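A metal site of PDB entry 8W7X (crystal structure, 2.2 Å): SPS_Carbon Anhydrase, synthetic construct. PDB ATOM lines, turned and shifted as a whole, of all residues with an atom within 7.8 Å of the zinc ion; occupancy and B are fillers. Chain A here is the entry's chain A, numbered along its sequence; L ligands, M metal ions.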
ATOM      1  N   TYR A   5      38.412 -26.988  25.504  1.00  0.00           N
ATOM      2  CA  TYR A   5      37.359 -27.978  25.620  1.00  0.00           C
ATOM      3  C   TYR A   5      37.888 -29.363  25.992  1.00  0.00           C
ATOM      4  O   TYR A   5      37.090 -30.297  26.102  1.00  0.00           O
ATOM      5  CB  TYR A   5      36.555 -28.057  24.319  1.00  0.00           C
ATOM      6  CG  TYR A   5      35.640 -26.858  24.093  1.00  0.00           C
ATOM      7  CD1 TYR A   5      34.400 -26.769  24.732  1.00  0.00           C
ATOM      8  CD2 TYR A   5      36.015 -25.811  23.238  1.00  0.00           C
ATOM      9  CE1 TYR A   5      33.551 -25.679  24.526  1.00  0.00           C
ATOM     10  CE2 TYR A   5      35.167 -24.713  23.026  1.00  0.00           C
ATOM     11  CZ  TYR A   5      33.938 -24.658  23.674  1.00  0.00           C
ATOM     12  OH  TYR A   5      33.100 -23.592  23.488  1.00  0.00           O
ATOM     13  N   THR A  65      35.832 -20.803  18.561  1.00  0.00           N
ATOM     14  CA  THR A  65      34.670 -20.753  17.685  1.00  0.00           C
ATOM     15  C   THR A  65      34.997 -19.765  16.569  1.00  0.00           C
ATOM     16  O   THR A  65      36.035 -19.095  16.587  1.00  0.00           O
ATOM     17  CB  THR A  65      33.403 -20.334  18.428  1.00  0.00           C
ATOM     18  OG1 THR A  65      32.284 -20.405  17.540  1.00  0.00           O
ATOM     19  CG2 THR A  65      33.529 -18.885  18.964  1.00  0.00           C
ATOM     20  N   GLN A  87      26.502 -10.494  18.259  1.00  0.00           N
ATOM     21  CA  GLN A  87      27.347 -11.428  17.535  1.00  0.00           C
ATOM     22  C   GLN A  87      26.619 -12.757  17.472  1.00  0.00           C
ATOM     23  O   GLN A  87      25.721 -13.023  18.269  1.00  0.00           O
ATOM     24  CB  GLN A  87      28.724 -11.603  18.219  1.00  0.00           C
ATOM     25  CG  GLN A  87      28.626 -11.931  19.721  1.00  0.00           C
ATOM     26  CD  GLN A  87      28.904 -13.396  20.073  1.00  0.00           C
ATOM     27  OE1 GLN A  87      28.684 -14.312  19.280  1.00  0.00           O
ATOM     28  NE2 GLN A  87      29.413 -13.603  21.261  1.00  0.00           N
ATOM     29  N   PHE A  88      27.007 -13.593  16.520  1.00  0.00           N
ATOM     30  CA  PHE A  88      26.612 -14.985  16.553  1.00  0.00           C
ATOM     31  C   PHE A  88      27.848 -15.833  16.278  1.00  0.00           C
ATOM     32  O   PHE A  88      28.855 -15.338  15.778  1.00  0.00           O
ATOM     33  CB  PHE A  88      25.457 -15.319  15.584  1.00  0.00           C
ATOM     34  CG  PHE A  88      25.725 -14.991  14.122  1.00  0.00           C
ATOM     35  CD1 PHE A  88      25.462 -13.720  13.608  1.00  0.00           C
ATOM     36  CD2 PHE A  88      26.211 -15.963  13.257  1.00  0.00           C
ATOM     37  CE1 PHE A  88      25.690 -13.422  12.259  1.00  0.00           C
ATOM     38  CE2 PHE A  88      26.453 -15.675  11.915  1.00  0.00           C
ATOM     39  CZ  PHE A  88      26.189 -14.402  11.418  1.00  0.00           C
ATOM     40  N   HIS A  89      27.794 -17.089  16.687  1.00  0.00           N
ATOM     41  CA  HIS A  89      28.944 -17.992  16.568  1.00  0.00           C
ATOM     42  C   HIS A  89      28.405 -19.409  16.581  1.00  0.00           C
ATOM     43  O   HIS A  89      27.196 -19.639  16.698  1.00  0.00           O
ATOM     44  CB  HIS A  89      29.954 -17.739  17.684  1.00  0.00           C
ATOM     45  CG  HIS A  89      29.395 -18.001  19.042  1.00  0.00           C
ATOM     46  ND1 HIS A  89      28.856 -17.007  19.818  1.00  0.00           N
ATOM     47  CD2 HIS A  89      29.223 -19.153  19.726  1.00  0.00           C
ATOM     48  CE1 HIS A  89      28.411 -17.527  20.939  1.00  0.00           C
ATOM     49  NE2 HIS A  89      28.632 -18.825  20.922  1.00  0.00           N
ATOM     50  N   PHE A  90      29.318 -20.389  16.492  1.00  0.00           N
ATOM     51  CA  PHE A  90      28.916 -21.751  16.112  1.00  0.00           C
ATOM     52  C   PHE A  90      29.586 -22.806  16.982  1.00  0.00           C
ATOM     53  O   PHE A  90      30.712 -22.638  17.444  1.00  0.00           O
ATOM     54  CB  PHE A  90      29.255 -21.992  14.614  1.00  0.00           C
ATOM     55  CG  PHE A  90      28.643 -20.993  13.703  1.00  0.00           C
ATOM     56  CD1 PHE A  90      27.332 -21.153  13.269  1.00  0.00           C
ATOM     57  CD2 PHE A  90      29.356 -19.884  13.276  1.00  0.00           C
ATOM     58  CE1 PHE A  90      26.741 -20.209  12.421  1.00  0.00           C
ATOM     59  CE2 PHE A  90      28.767 -18.930  12.438  1.00  0.00           C
ATOM     60  CZ  PHE A  90      27.470 -19.093  12.005  1.00  0.00           C
ATOM     61  N   HIS A  91      28.880 -23.927  17.149  1.00  0.00           N
ATOM     62  CA  HIS A  91      29.383 -25.084  17.860  1.00  0.00           C
ATOM     63  C   HIS A  91      29.102 -26.345  17.058  1.00  0.00           C
ATOM     64  O   HIS A  91      28.036 -26.491  16.460  1.00  0.00           O
ATOM     65  CB  HIS A  91      28.753 -25.211  19.259  1.00  0.00           C
ATOM     66  CG  HIS A  91      28.975 -24.022  20.136  1.00  0.00           C
ATOM     67  ND1 HIS A  91      30.147 -23.813  20.839  1.00  0.00           N
ATOM     68  CD2 HIS A  91      28.176 -22.967  20.438  1.00  0.00           C
ATOM     69  CE1 HIS A  91      30.059 -22.677  21.519  1.00  0.00           C
ATOM     70  NE2 HIS A  91      28.868 -22.156  21.296  1.00  0.00           N
ATOM     71  N   GLU A  95      25.527 -27.905  21.216  1.00  0.00           N
ATOM     72  CA  GLU A  95      25.667 -27.832  22.664  1.00  0.00           C
ATOM     73  C   GLU A  95      24.460 -28.443  23.354  1.00  0.00           C
ATOM     74  O   GLU A  95      24.589 -29.386  24.140  1.00  0.00           O
ATOM     75  CB  GLU A  95      25.893 -26.388  23.084  1.00  0.00           C
ATOM     76  CG  GLU A  95      27.238 -25.929  22.621  1.00  0.00           C
ATOM     77  CD  GLU A  95      27.896 -24.973  23.535  1.00  0.00           C
ATOM     78  OE1 GLU A  95      27.271 -23.946  23.874  1.00  0.00           O
ATOM     79  OE2 GLU A  95      29.058 -25.238  23.915  1.00  0.00           O
ATOM     80  N   GLU A 106      25.255 -26.082  15.713  1.00  0.00           N
ATOM     81  CA  GLU A 106      24.379 -25.176  16.446  1.00  0.00           C
ATOM     82  C   GLU A 106      24.927 -23.755  16.345  1.00  0.00           C
ATOM     83  O   GLU A 106      26.132 -23.538  16.537  1.00  0.00           O
ATOM     84  CB  GLU A 106      24.256 -25.593  17.933  1.00  0.00           C
ATOM     85  CG  GLU A 106      23.317 -24.732  18.821  1.00  0.00           C
ATOM     86  CD  GLU A 106      23.156 -25.301  20.264  1.00  0.00           C
ATOM     87  OE1 GLU A 106      23.370 -26.519  20.477  1.00  0.00           O
ATOM     88  OE2 GLU A 106      22.830 -24.539  21.199  1.00  0.00           O
ATOM     89  N   ALA A 107      24.042 -22.793  16.093  1.00  0.00           N
ATOM     90  CA  ALA A 107      24.381 -21.382  16.105  1.00  0.00           C
ATOM     91  C   ALA A 107      23.783 -20.690  17.337  1.00  0.00           C
ATOM     92  O   ALA A 107      22.638 -20.970  17.713  1.00  0.00           O
ATOM     93  CB  ALA A 107      23.865 -20.691  14.832  1.00  0.00           C
ATOM     94  N   HIS A 108      24.557 -19.796  17.949  1.00  0.00           N
ATOM     95  CA  HIS A 108      24.094 -18.985  19.078  1.00  0.00           C
ATOM     96  C   HIS A 108      24.114 -17.525  18.685  1.00  0.00           C
ATOM     97  O   HIS A 108      25.144 -17.012  18.271  1.00  0.00           O
ATOM     98  CB  HIS A 108      24.970 -19.151  20.319  1.00  0.00           C
ATOM     99  CG  HIS A 108      24.916 -20.513  20.929  1.00  0.00           C
ATOM    100  ND1 HIS A 108      25.916 -20.987  21.751  1.00  0.00           N
ATOM    101  CD2 HIS A 108      23.985 -21.499  20.835  1.00  0.00           C
ATOM    102  CE1 HIS A 108      25.603 -22.211  22.146  1.00  0.00           C
ATOM    103  NE2 HIS A 108      24.443 -22.548  21.589  1.00  0.00           N
ATOM    104  N   PHE A 109      22.973 -16.856  18.826  1.00  0.00           N
ATOM    105  CA  PHE A 109      22.846 -15.426  18.564  1.00  0.00           C
ATOM    106  C   PHE A 109      22.804 -14.713  19.915  1.00  0.00           C
ATOM    107  O   PHE A 109      21.823 -14.842  20.660  1.00  0.00           O
ATOM    108  CB  PHE A 109      21.608 -15.167  17.704  1.00  0.00           C
ATOM    109  CG  PHE A 109      21.631 -15.917  16.369  1.00  0.00           C
ATOM    110  CD1 PHE A 109      21.342 -17.272  16.306  1.00  0.00           C
ATOM    111  CD2 PHE A 109      22.013 -15.266  15.208  1.00  0.00           C
ATOM    112  CE1 PHE A 109      21.392 -17.967  15.117  1.00  0.00           C
ATOM    113  CE2 PHE A 109      22.064 -15.955  13.994  1.00  0.00           C
ATOM    114  CZ  PHE A 109      21.753 -17.309  13.961  1.00  0.00           C
ATOM    115  N   VAL A 110      23.868 -13.981  20.240  1.00  0.00           N
ATOM    116  CA  VAL A 110      24.044 -13.414  21.573  1.00  0.00           C
ATOM    117  C   VAL A 110      23.563 -11.959  21.583  1.00  0.00           C
ATOM    118  O   VAL A 110      24.018 -11.144  20.778  1.00  0.00           O
ATOM    119  CB  VAL A 110      25.508 -13.532  22.043  1.00  0.00           C
ATOM    120  CG1 VAL A 110      25.687 -12.875  23.421  1.00  0.00           C
ATOM    121  CG2 VAL A 110      25.922 -15.010  22.105  1.00  0.00           C
ATOM    122  N   VAL A 120      20.203 -15.381  24.632  1.00  0.00           N
ATOM    123  CA  VAL A 120      20.844 -16.127  23.544  1.00  0.00           C
ATOM    124  C   VAL A 120      19.788 -16.947  22.809  1.00  0.00           C
ATOM    125  O   VAL A 120      19.011 -17.663  23.438  1.00  0.00           O
ATOM    126  CB  VAL A 120      21.975 -17.036  24.062  1.00  0.00           C
ATOM    127  CG1 VAL A 120      22.715 -17.670  22.871  1.00  0.00           C
ATOM    128  CG2 VAL A 120      22.922 -16.231  24.903  1.00  0.00           C
ATOM    129  N   ILE A 121      19.754 -16.823  21.482  1.00  0.00           N
ATOM    130  CA  ILE A 121      18.936 -17.681  20.629  1.00  0.00           C
ATOM    131  C   ILE A 121      19.825 -18.783  20.070  1.00  0.00           C
ATOM    132  O   ILE A 121      20.885 -18.511  19.503  1.00  0.00           O
ATOM    133  CB  ILE A 121      18.258 -16.901  19.500  1.00  0.00           C
ATOM    134  CG1 ILE A 121      17.210 -15.945  20.066  1.00  0.00           C
ATOM    135  CG2 ILE A 121      17.643 -17.862  18.493  1.00  0.00           C
ATOM    136  CD1 ILE A 121      16.606 -15.007  19.039  1.00  0.00           C
ATOM    137  N   LEU A 174      25.992 -18.494  30.117  1.00  0.00           N
ATOM    138  CA  LEU A 174      26.946 -18.625  29.019  1.00  0.00           C
ATOM    139  C   LEU A 174      27.554 -20.030  29.039  1.00  0.00           C
ATOM    140  O   LEU A 174      27.726 -20.634  30.102  1.00  0.00           O
ATOM    141  CB  LEU A 174      28.054 -17.580  29.159  1.00  0.00           C
ATOM    142  CG  LEU A 174      27.536 -16.138  29.118  1.00  0.00           C
ATOM    143  CD1 LEU A 174      28.671 -15.161  29.414  1.00  0.00           C
ATOM    144  CD2 LEU A 174      26.892 -15.880  27.769  1.00  0.00           C
ATOM    145  N   THR A 175      27.881 -20.541  27.855  1.00  0.00           N
ATOM    146  CA  THR A 175      28.461 -21.880  27.794  1.00  0.00           C
ATOM    147  C   THR A 175      29.971 -21.877  27.656  1.00  0.00           C
ATOM    148  O   THR A 175      30.576 -22.946  27.559  1.00  0.00           O
ATOM    149  CB  THR A 175      27.842 -22.700  26.658  1.00  0.00           C
ATOM    150  OG1 THR A 175      28.166 -22.122  25.388  1.00  0.00           O
ATOM    151  CG2 THR A 175      26.327 -22.743  26.812  1.00  0.00           C
ATOM    152  N   THR A 176      30.590 -20.700  27.681  1.00  0.00           N
ATOM    153  CA  THR A 176      32.028 -20.565  27.810  1.00  0.00           C
ATOM    154  C   THR A 176      32.334 -19.682  29.022  1.00  0.00           C
ATOM    155  O   THR A 176      31.475 -18.888  29.457  1.00  0.00           O
ATOM    156  CB  THR A 176      32.634 -19.949  26.546  1.00  0.00           C
ATOM    157  OG1 THR A 176      32.088 -18.642  26.343  1.00  0.00           O
ATOM    158  CG2 THR A 176      32.359 -20.812  25.315  1.00  0.00           C
ATOM    159  N   TRP A 185      17.689 -18.307  27.732  1.00  0.00           N
ATOM    160  CA  TRP A 185      17.920 -19.160  26.568  1.00  0.00           C
ATOM    161  C   TRP A 185      16.628 -19.367  25.790  1.00  0.00           C
ATOM    162  O   TRP A 185      15.584 -19.685  26.367  1.00  0.00           O
ATOM    163  CB  TRP A 185      18.509 -20.515  26.984  1.00  0.00           C
ATOM    164  CG  TRP A 185      19.978 -20.422  27.098  1.00  0.00           C
ATOM    165  CD1 TRP A 185      20.690 -20.106  28.215  1.00  0.00           C
ATOM    166  CD2 TRP A 185      20.943 -20.576  26.037  1.00  0.00           C
ATOM    167  NE1 TRP A 185      22.033 -20.081  27.925  1.00  0.00           N
ATOM    168  CE2 TRP A 185      22.216 -20.366  26.599  1.00  0.00           C
ATOM    169  CE3 TRP A 185      20.842 -20.865  24.666  1.00  0.00           C
ATOM    170  CZ2 TRP A 185      23.401 -20.443  25.843  1.00  0.00           C
ATOM    171  CZ3 TRP A 185      21.996 -20.962  23.929  1.00  0.00           C
ATOM    172  CH2 TRP A 185      23.270 -20.741  24.520  1.00  0.00           C
ATOM    173  N   ASN A 210      33.946 -28.431  19.828  1.00  0.00           N
ATOM    174  CA  ASN A 210      33.964 -27.175  20.555  1.00  0.00           C
ATOM    175  C   ASN A 210      32.619 -26.940  21.257  1.00  0.00           C
ATOM    176  O   ASN A 210      32.099 -25.826  21.280  1.00  0.00           O
ATOM    177  CB  ASN A 210      34.338 -26.019  19.627  1.00  0.00           C
ATOM    178  CG  ASN A 210      33.210 -25.610  18.695  1.00  0.00           C
ATOM    179  OD1 ASN A 210      32.428 -26.442  18.216  1.00  0.00           O
ATOM    180  ND2 ASN A 210      33.098 -24.303  18.445  1.00  0.00           N
HETATM  181  C1  LIG L   1      27.207 -19.169  24.656  1.00  0.00           C
HETATM  182  O1  LIG L   1      28.007 -20.042  24.227  1.00  0.00           O
HETATM  183  O2  LIG L   1      27.214 -18.421  25.637  1.00  0.00           O
HETATM  184  O3  LIG L   1      26.389 -18.667  23.598  1.00  0.00           O
HETATM  185 ZN    ZN M   1      27.874 -20.471  22.058  1.00  0.00          ZN
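The zinc ion is bound by a ring nitrogen (ND1) of His 108 (2.0 Å), a ring nitrogen (NE2) of His 91 (2.1 Å), a ring nitrogen (NE2) of His 89 (2.1 Å) and an oxygen (O1) of the ligand (2.2 Å).
Slightly farther from the zinc ion lies an oxygen (O3) of the ligand (2.8 Å).
OE1 of Gln 87 sits at hydrogen-bond distance from ND1 of His 89 (2.8 Å).
The backbone NH of Glu 95 lies within hydrogen-bond range of the side-chain carboxylate of Glu 106 (2.7 Å).
The backbone carbonyl oxygen (O) of Asn 210 is in hydrogen-bond range of a ring nitrogen (ND1) of His 91, at 2.8 Å.
The side-chain carboxylate (OE1) of Glu 95 lies within hydrogen-bond range of the side-chain hydroxyl (OG1) of Thr 175 (2.5 Å).
The backbone NH of His 91 is in hydrogen-bond range of the backbone carbonyl oxygen of Glu 106, at 2.8 Å.
A ring nitrogen (NE2) of His 108 is in hydrogen-bond range of the side-chain carboxylate of Glu 106, 2.6 Å away.
Glu 95 touches the zinc ion (OE1 to ZN, 3.97 Å).
Thr 175 touches the zinc ion.
Within 4 Å of the zinc ion: His 89, His 91, Glu 95, His 108 and Thr 175.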
